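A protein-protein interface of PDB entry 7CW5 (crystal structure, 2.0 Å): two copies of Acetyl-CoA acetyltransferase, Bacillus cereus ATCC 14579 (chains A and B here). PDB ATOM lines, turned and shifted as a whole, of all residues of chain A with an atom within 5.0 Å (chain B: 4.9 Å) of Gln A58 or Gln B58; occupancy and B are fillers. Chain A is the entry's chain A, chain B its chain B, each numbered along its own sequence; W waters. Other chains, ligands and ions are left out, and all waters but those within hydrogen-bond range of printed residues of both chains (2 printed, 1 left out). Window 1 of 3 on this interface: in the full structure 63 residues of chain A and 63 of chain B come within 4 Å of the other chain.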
ATOM      1  N   THR A  55     -18.851 -23.627  10.388  1.00  0.00           N
ATOM      2  CA  THR A  55     -20.168 -24.064   9.867  1.00  0.00           C
ATOM      3  C   THR A  55     -20.036 -25.533   9.518  1.00  0.00           C
ATOM      4  O   THR A  55     -18.957 -25.927   8.978  1.00  0.00           O
ATOM      5  CB  THR A  55     -20.639 -23.194   8.701  1.00  0.00           C
ATOM      6  OG1 THR A  55     -22.010 -23.497   8.438  1.00  0.00           O
ATOM      7  CG2 THR A  55     -19.841 -23.406   7.433  1.00  0.00           C
ATOM      8  N   VAL A  56     -21.092 -26.296   9.769  1.00  0.00           N
ATOM      9  CA  VAL A  56     -21.018 -27.778   9.689  1.00  0.00           C
ATOM     10  C   VAL A  56     -21.608 -28.271   8.373  1.00  0.00           C
ATOM     11  O   VAL A  56     -20.964 -29.126   7.722  1.00  0.00           O
ATOM     12  CB  VAL A  56     -21.695 -28.414  10.903  1.00  0.00           C
ATOM     13  CG1 VAL A  56     -21.684 -29.945  10.805  1.00  0.00           C
ATOM     14  CG2 VAL A  56     -21.031 -27.920  12.174  1.00  0.00           C
ATOM     15  N   ILE A  57     -22.790 -27.788   8.004  1.00  0.00           N
ATOM     16  CA  ILE A  57     -23.480 -28.304   6.788  1.00  0.00           C
ATOM     17  C   ILE A  57     -23.087 -27.373   5.633  1.00  0.00           C
ATOM     18  O   ILE A  57     -23.857 -26.489   5.278  1.00  0.00           O
ATOM     19  CB  ILE A  57     -24.993 -28.430   7.025  1.00  0.00           C
ATOM     20  CG1 ILE A  57     -25.312 -29.205   8.312  1.00  0.00           C
ATOM     21  CG2 ILE A  57     -25.688 -29.047   5.811  1.00  0.00           C
ATOM     22  CD1 ILE A  57     -24.897 -30.661   8.308  1.00  0.00           C
ATOM     23  N   GLN A  58     -21.878 -27.546   5.116  1.00  0.00           N
ATOM     24  CA  GLN A  58     -21.275 -26.627   4.110  1.00  0.00           C
ATOM     25  C   GLN A  58     -21.830 -26.905   2.720  1.00  0.00           C
ATOM     26  O   GLN A  58     -21.828 -25.971   1.883  1.00  0.00           O
ATOM     27  CB  GLN A  58     -19.761 -26.790   4.094  1.00  0.00           C
ATOM     28  CG  GLN A  58     -19.176 -26.319   5.403  1.00  0.00           C
ATOM     29  CD  GLN A  58     -17.677 -26.319   5.436  1.00  0.00           C
ATOM     30  OE1 GLN A  58     -17.005 -26.384   4.396  1.00  0.00           O
ATOM     31  NE2 GLN A  58     -17.169 -26.313   6.658  1.00  0.00           N
ATOM     32  N   GLY A  59     -22.285 -28.133   2.482  1.00  0.00           N
ATOM     33  CA  GLY A  59     -22.819 -28.527   1.172  1.00  0.00           C
ATOM     34  C   GLY A  59     -23.853 -27.539   0.677  1.00  0.00           C
ATOM     35  O   GLY A  59     -24.928 -27.425   1.285  1.00  0.00           O
ATOM     36  N   GLY A  60     -23.532 -26.852  -0.408  1.00  0.00           N
ATOM     37  CA  GLY A  60     -24.465 -25.955  -1.097  1.00  0.00           C
ATOM     38  C   GLY A  60     -24.381 -24.535  -0.591  1.00  0.00           C
ATOM     39  O   GLY A  60     -25.061 -23.694  -1.174  1.00  0.00           O
ATOM     40  N   GLN A  61     -23.516 -24.241   0.386  1.00  0.00           N
ATOM     41  CA  GLN A  61     -23.323 -22.847   0.853  1.00  0.00           C
ATOM     42  C   GLN A  61     -22.474 -22.037  -0.123  1.00  0.00           C
ATOM     43  O   GLN A  61     -22.464 -20.796   0.028  1.00  0.00           O
ATOM     44  CB  GLN A  61     -22.680 -22.858   2.226  1.00  0.00           C
ATOM     45  CG  GLN A  61     -23.621 -23.388   3.281  1.00  0.00           C
ATOM     46  CD  GLN A  61     -23.188 -22.938   4.652  1.00  0.00           C
ATOM     47  OE1 GLN A  61     -23.098 -23.708   5.599  1.00  0.00           O
ATOM     48  NE2 GLN A  61     -22.946 -21.656   4.762  1.00  0.00           N
ATOM     49  N   GLY A  62     -21.762 -22.707  -1.055  1.00  0.00           N
ATOM     50  CA  GLY A  62     -20.822 -22.057  -1.978  1.00  0.00           C
ATOM     51  C   GLY A  62     -19.414 -22.008  -1.411  1.00  0.00           C
ATOM     52  O   GLY A  62     -19.198 -22.430  -0.233  1.00  0.00           O
ATOM     53  N   PRO A  65     -17.462 -20.558   2.872  1.00  0.00           N
ATOM     54  CA  PRO A  65     -18.506 -19.803   3.560  1.00  0.00           C
ATOM     55  C   PRO A  65     -18.001 -18.693   4.485  1.00  0.00           C
ATOM     56  O   PRO A  65     -18.703 -17.680   4.590  1.00  0.00           O
ATOM     57  CB  PRO A  65     -19.269 -20.905   4.306  1.00  0.00           C
ATOM     58  CG  PRO A  65     -19.082 -22.127   3.428  1.00  0.00           C
ATOM     59  CD  PRO A  65     -17.680 -22.013   2.911  1.00  0.00           C
ATOM     60  N   THR A  83     -12.713 -21.484   6.727  1.00  0.00           N
ATOM     61  CA  THR A  83     -13.892 -22.132   7.340  1.00  0.00           C
ATOM     62  C   THR A  83     -13.438 -23.399   8.091  1.00  0.00           C
ATOM     63  O   THR A  83     -12.648 -24.240   7.537  1.00  0.00           O
ATOM     64  CB  THR A  83     -14.933 -22.428   6.252  1.00  0.00           C
ATOM     65  OG1 THR A  83     -15.084 -21.243   5.481  1.00  0.00           O
ATOM     66  CG2 THR A  83     -16.252 -22.879   6.818  1.00  0.00           C
ATOM     67  N   VAL A  84     -13.926 -23.577   9.306  1.00  0.00           N
ATOM     68  CA  VAL A  84     -13.530 -24.727  10.147  1.00  0.00           C
ATOM     69  C   VAL A  84     -14.762 -25.568  10.455  1.00  0.00           C
ATOM     70  O   VAL A  84     -15.867 -25.015  10.652  1.00  0.00           O
ATOM     71  CB  VAL A  84     -12.816 -24.266  11.437  1.00  0.00           C
ATOM     72  CG1 VAL A  84     -11.541 -23.517  11.119  1.00  0.00           C
ATOM     73  CG2 VAL A  84     -13.710 -23.408  12.329  1.00  0.00           C
ATOM     74  N   ASN A  85     -14.547 -26.861  10.596  1.00  0.00           N
ATOM     75  CA  ASN A  85     -15.628 -27.825  10.888  1.00  0.00           C
ATOM     76  C   ASN A  85     -15.129 -28.743  11.996  1.00  0.00           C
ATOM     77  O   ASN A  85     -14.199 -29.535  11.725  1.00  0.00           O
ATOM     78  CB  ASN A  85     -16.057 -28.562   9.610  1.00  0.00           C
ATOM     79  CG  ASN A  85     -17.152 -29.593   9.830  1.00  0.00           C
ATOM     80  OD1 ASN A  85     -17.602 -29.815  10.955  1.00  0.00           O
ATOM     81  ND2 ASN A  85     -17.595 -30.225   8.753  1.00  0.00           N
ATOM     82  N   ASP A 146     -24.613 -35.238   7.184  1.00  0.00           N
ATOM     83  CA  ASP A 146     -23.351 -34.533   7.519  1.00  0.00           C
ATOM     84  C   ASP A 146     -23.401 -34.004   8.953  1.00  0.00           C
ATOM     85  O   ASP A 146     -22.344 -33.594   9.428  1.00  0.00           O
ATOM     86  CB  ASP A 146     -23.036 -33.443   6.491  1.00  0.00           C
ATOM     87  CG  ASP A 146     -22.555 -34.002   5.140  1.00  0.00           C
ATOM     88  OD1 ASP A 146     -22.368 -35.225   5.040  1.00  0.00           O
ATOM     89  OD2 ASP A 146     -22.397 -33.211   4.184  1.00  0.00           O
ATOM     90  N   THR B  55     -10.447 -30.408   3.274  1.00  0.00           N
ATOM     91  CA  THR B  55     -11.287 -30.922   2.146  1.00  0.00           C
ATOM     92  C   THR B  55     -12.341 -29.865   1.840  1.00  0.00           C
ATOM     93  O   THR B  55     -12.801 -29.195   2.804  1.00  0.00           O
ATOM     94  CB  THR B  55     -11.833 -32.323   2.444  1.00  0.00           C
ATOM     95  OG1 THR B  55     -12.358 -32.899   1.245  1.00  0.00           O
ATOM     96  CG2 THR B  55     -12.915 -32.329   3.495  1.00  0.00           C
ATOM     97  N   VAL B  56     -12.677 -29.715   0.560  1.00  0.00           N
ATOM     98  CA  VAL B  56     -13.468 -28.569   0.035  1.00  0.00           C
ATOM     99  C   VAL B  56     -14.904 -29.006  -0.239  1.00  0.00           C
ATOM    100  O   VAL B  56     -15.832 -28.339   0.247  1.00  0.00           O
ATOM    101  CB  VAL B  56     -12.817 -27.988  -1.224  1.00  0.00           C
ATOM    102  CG1 VAL B  56     -13.689 -26.857  -1.797  1.00  0.00           C
ATOM    103  CG2 VAL B  56     -11.410 -27.521  -0.882  1.00  0.00           C
ATOM    104  N   ILE B  57     -15.091 -30.108  -0.948  1.00  0.00           N
ATOM    105  CA  ILE B  57     -16.476 -30.565  -1.258  1.00  0.00           C
ATOM    106  C   ILE B  57     -16.919 -31.526  -0.139  1.00  0.00           C
ATOM    107  O   ILE B  57     -16.909 -32.728  -0.322  1.00  0.00           O
ATOM    108  CB  ILE B  57     -16.540 -31.132  -2.675  1.00  0.00           C
ATOM    109  CG1 ILE B  57     -15.839 -30.205  -3.675  1.00  0.00           C
ATOM    110  CG2 ILE B  57     -17.984 -31.410  -3.072  1.00  0.00           C
ATOM    111  CD1 ILE B  57     -16.422 -28.806  -3.755  1.00  0.00           C
ATOM    112  N   GLN B  58     -17.246 -30.966   1.028  1.00  0.00           N
ATOM    113  CA  GLN B  58     -17.588 -31.726   2.260  1.00  0.00           C
ATOM    114  C   GLN B  58     -18.986 -32.320   2.158  1.00  0.00           C
ATOM    115  O   GLN B  58     -19.243 -33.288   2.896  1.00  0.00           O
ATOM    116  CB  GLN B  58     -17.518 -30.845   3.493  1.00  0.00           C
ATOM    117  CG  GLN B  58     -16.114 -30.334   3.714  1.00  0.00           C
ATOM    118  CD  GLN B  58     -15.930 -29.500   4.954  1.00  0.00           C
ATOM    119  OE1 GLN B  58     -16.815 -29.416   5.803  1.00  0.00           O
ATOM    120  NE2 GLN B  58     -14.764 -28.863   5.035  1.00  0.00           N
ATOM    121  N   GLY B  59     -19.851 -31.737   1.329  1.00  0.00           N
ATOM    122  CA  GLY B  59     -21.234 -32.188   1.118  1.00  0.00           C
ATOM    123  C   GLY B  59     -21.305 -33.676   0.832  1.00  0.00           C
ATOM    124  O   GLY B  59     -20.812 -34.112  -0.224  1.00  0.00           O
ATOM    125  N   GLY B  60     -21.854 -34.425   1.779  1.00  0.00           N
ATOM    126  CA  GLY B  60     -22.119 -35.861   1.637  1.00  0.00           C
ATOM    127  C   GLY B  60     -20.978 -36.717   2.110  1.00  0.00           C
ATOM    128  O   GLY B  60     -21.128 -37.947   2.042  1.00  0.00           O
ATOM    129  N   GLN B  61     -19.869 -36.128   2.571  1.00  0.00           N
ATOM    130  CA  GLN B  61     -18.743 -36.921   3.134  1.00  0.00           C
ATOM    131  C   GLN B  61     -19.080 -37.466   4.523  1.00  0.00           C
ATOM    132  O   GLN B  61     -18.380 -38.352   4.977  1.00  0.00           O
ATOM    133  CB  GLN B  61     -17.478 -36.075   3.207  1.00  0.00           C
ATOM    134  CG  GLN B  61     -16.845 -35.928   1.836  1.00  0.00           C
ATOM    135  CD  GLN B  61     -15.430 -35.422   1.920  1.00  0.00           C
ATOM    136  OE1 GLN B  61     -15.128 -34.340   1.420  1.00  0.00           O
ATOM    137  NE2 GLN B  61     -14.567 -36.206   2.539  1.00  0.00           N
ATOM    138  N   GLY B  62     -20.073 -36.894   5.206  1.00  0.00           N
ATOM    139  CA  GLY B  62     -20.422 -37.295   6.561  1.00  0.00           C
ATOM    140  C   GLY B  62     -19.722 -36.436   7.585  1.00  0.00           C
ATOM    141  O   GLY B  62     -18.863 -35.582   7.207  1.00  0.00           O
ATOM    142  N   PRO B  65     -15.030 -34.880   8.292  1.00  0.00           N
ATOM    143  CA  PRO B  65     -14.219 -35.774   7.452  1.00  0.00           C
ATOM    144  C   PRO B  65     -12.781 -36.006   7.945  1.00  0.00           C
ATOM    145  O   PRO B  65     -12.289 -37.095   7.749  1.00  0.00           O
ATOM    146  CB  PRO B  65     -14.229 -35.095   6.072  1.00  0.00           C
ATOM    147  CG  PRO B  65     -15.496 -34.252   6.082  1.00  0.00           C
ATOM    148  CD  PRO B  65     -15.696 -33.826   7.514  1.00  0.00           C
ATOM    149  N   THR B  83     -11.632 -30.330  10.582  1.00  0.00           N
ATOM    150  CA  THR B  83     -11.582 -30.205   9.122  1.00  0.00           C
ATOM    151  C   THR B  83     -11.516 -28.717   8.794  1.00  0.00           C
ATOM    152  O   THR B  83     -12.350 -27.894   9.356  1.00  0.00           O
ATOM    153  CB  THR B  83     -12.792 -30.910   8.518  1.00  0.00           C
ATOM    154  OG1 THR B  83     -12.838 -32.215   9.101  1.00  0.00           O
ATOM    155  CG2 THR B  83     -12.716 -30.958   7.024  1.00  0.00           C
ATOM    156  N   VAL B  84     -10.638 -28.372   7.874  1.00  0.00           N
ATOM    157  CA  VAL B  84     -10.511 -26.971   7.416  1.00  0.00           C
ATOM    158  C   VAL B  84     -10.816 -26.867   5.922  1.00  0.00           C
ATOM    159  O   VAL B  84     -10.577 -27.816   5.124  1.00  0.00           O
ATOM    160  CB  VAL B  84      -9.136 -26.384   7.788  1.00  0.00           C
ATOM    161  CG1 VAL B  84      -8.904 -26.429   9.285  1.00  0.00           C
ATOM    162  CG2 VAL B  84      -8.002 -27.083   7.047  1.00  0.00           C
ATOM    163  N   ASN B  85     -11.314 -25.699   5.546  1.00  0.00           N
ATOM    164  CA  ASN B  85     -11.655 -25.376   4.142  1.00  0.00           C
ATOM    165  C   ASN B  85     -11.156 -23.962   3.865  1.00  0.00           C
ATOM    166  O   ASN B  85     -11.701 -22.988   4.472  1.00  0.00           O
ATOM    167  CB  ASN B  85     -13.149 -25.594   3.900  1.00  0.00           C
ATOM    168  CG  ASN B  85     -13.659 -25.133   2.551  1.00  0.00           C
ATOM    169  OD1 ASN B  85     -12.910 -24.633   1.712  1.00  0.00           O
ATOM    170  ND2 ASN B  85     -14.953 -25.296   2.331  1.00  0.00           N
ATOM    171  N   ASP B 146     -19.792 -25.609  -4.918  1.00  0.00           N
ATOM    172  CA  ASP B 146     -18.928 -25.351  -3.731  1.00  0.00           C
ATOM    173  C   ASP B 146     -17.445 -25.224  -4.112  1.00  0.00           C
ATOM    174  O   ASP B 146     -16.664 -24.761  -3.270  1.00  0.00           O
ATOM    175  CB  ASP B 146     -19.192 -26.439  -2.688  1.00  0.00           C
ATOM    176  CG  ASP B 146     -20.547 -26.297  -2.017  1.00  0.00           C
ATOM    177  OD1 ASP B 146     -21.194 -25.213  -2.178  1.00  0.00           O
ATOM    178  OD2 ASP B 146     -20.975 -27.287  -1.358  1.00  0.00           O
HETATM  179  O   HOH W   1     -19.641 -30.005   5.814  1.00  0.00           O
HETATM  180  O   HOH W   2     -17.688 -27.559   1.873  1.00  0.00           O
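OD2 of Asp A146 lies within hydrogen-bond range of N of Gly B60 (2.7 Å). OE1 of Gln B58 sits at hydrogen-bond distance from ND2 of Asn A85, 3.2 Å away. OD2 of Asp A146 lies close to O of Gln B58, at 3.4 Å. OD1 of Asp A146 lies within hydrogen-bond range of N of Gly B62 (2.8 Å). N of Asn A85 is in hydrogen-bond range of O of Thr B83, 2.7 Å away. The side-chain amide oxygen (OE1) of Gln B58 lies close to the side-chain amide nitrogen (NE2) of Gln A58, 3.2 Å away. The side-chain amide oxygen of Gln A58 sits at hydrogen-bond distance from the side-chain amide nitrogen of Asn B85, 3.1 Å away. The backbone NH of Gly A62 lies within hydrogen-bond range of the side-chain carboxylate of Asp B146 (2.8 Å). O of Thr A83 lies within hydrogen-bond range of N of Asn B85 (2.8 Å). N of Gly A60 sits at hydrogen-bond distance from OD2 of Asp B146, 2.8 Å away.
Gln A58 touches Asn B85, and with the chains exchanged Asn A85 touches Gln B58. Gln A58 touches Asp B146, and with the chains exchanged Asp A146 touches Gln B58. Gly B59 touches its own counterpart, Gly A59. Gly A60 touches Asp B146, and with the chains exchanged Asp A146 touches Gly B60.
Water W1 lies within hydrogen-bond range of the backbone carbonyl oxygen (O) of Val A56 (2.5 Å), the side-chain amide oxygen (OE1) of Gln B58 (2.9 Å) and the backbone NH (N) of Gln A58 (3.4 Å). Water W2 lies within hydrogen-bond range of O of Val B56 (2.6 Å) and OE1 of Gln A58 (2.9 Å).
Among the printed residues, no Asp or Glu carboxylate lies within 4 Å of a Lys or Arg side-chain nitrogen of the other chain.
Gln A58 touches just these residues of chain B: Gln B58, Asn B85 and Asp B146. Gln B58 touches just these residues of chain A: Gln A58 (3.2 Å), Asn A85 (3.2 Å) and Asp A146 (3.4 Å). Of the printed residues of chain B, Gly A59 touches Gly B59 and Asp B146. Printed residues of chain B within 4 Å of Gly A62: Asp B146 (2.8 Å). Thr A55 touches none of the printed residues of chain B. Pro A65 touches none of the printed residues of chain B.
The side-chain hydroxyl of Thr B55 lies within hydrogen-bond range of the side-chain amide oxygen of Gln B61, at 3.1 Å. N of Thr B55 sits at hydrogen-bond distance from O of Val B84 (3.2 Å). The backbone carbonyl oxygen of Thr B55 lies within hydrogen-bond range of the side-chain amide nitrogen of Gln B58 (3.0 Å). N of Thr A55 sits at hydrogen-bond distance from O of Val A84, 3.3 Å away. The side-chain amide oxygen of Gln A61 sits close to the backbone carbonyl oxygen of Ile A57, at 2.9 Å. The side-chain amide oxygen of Gln B61 lies close to the backbone carbonyl oxygen of Ile B57 (3.0 Å).
Among the printed residues, merely in contact across the chains: Gly A59 with Asp B146 (3.4 Å), Asp A146 with Gly B59 (3.4 Å), Thr A83 with Val B84 (3.5 Å), Val A84 with Thr B83 (3.5 Å), Gln A61 with Asp B146 (3.6 Å), Gln A58 with Asp B146 (3.6 Å), Asp A146 with Gln B61 (3.6 Å) and Gly A59 with Gly B59 (3.99 Å).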
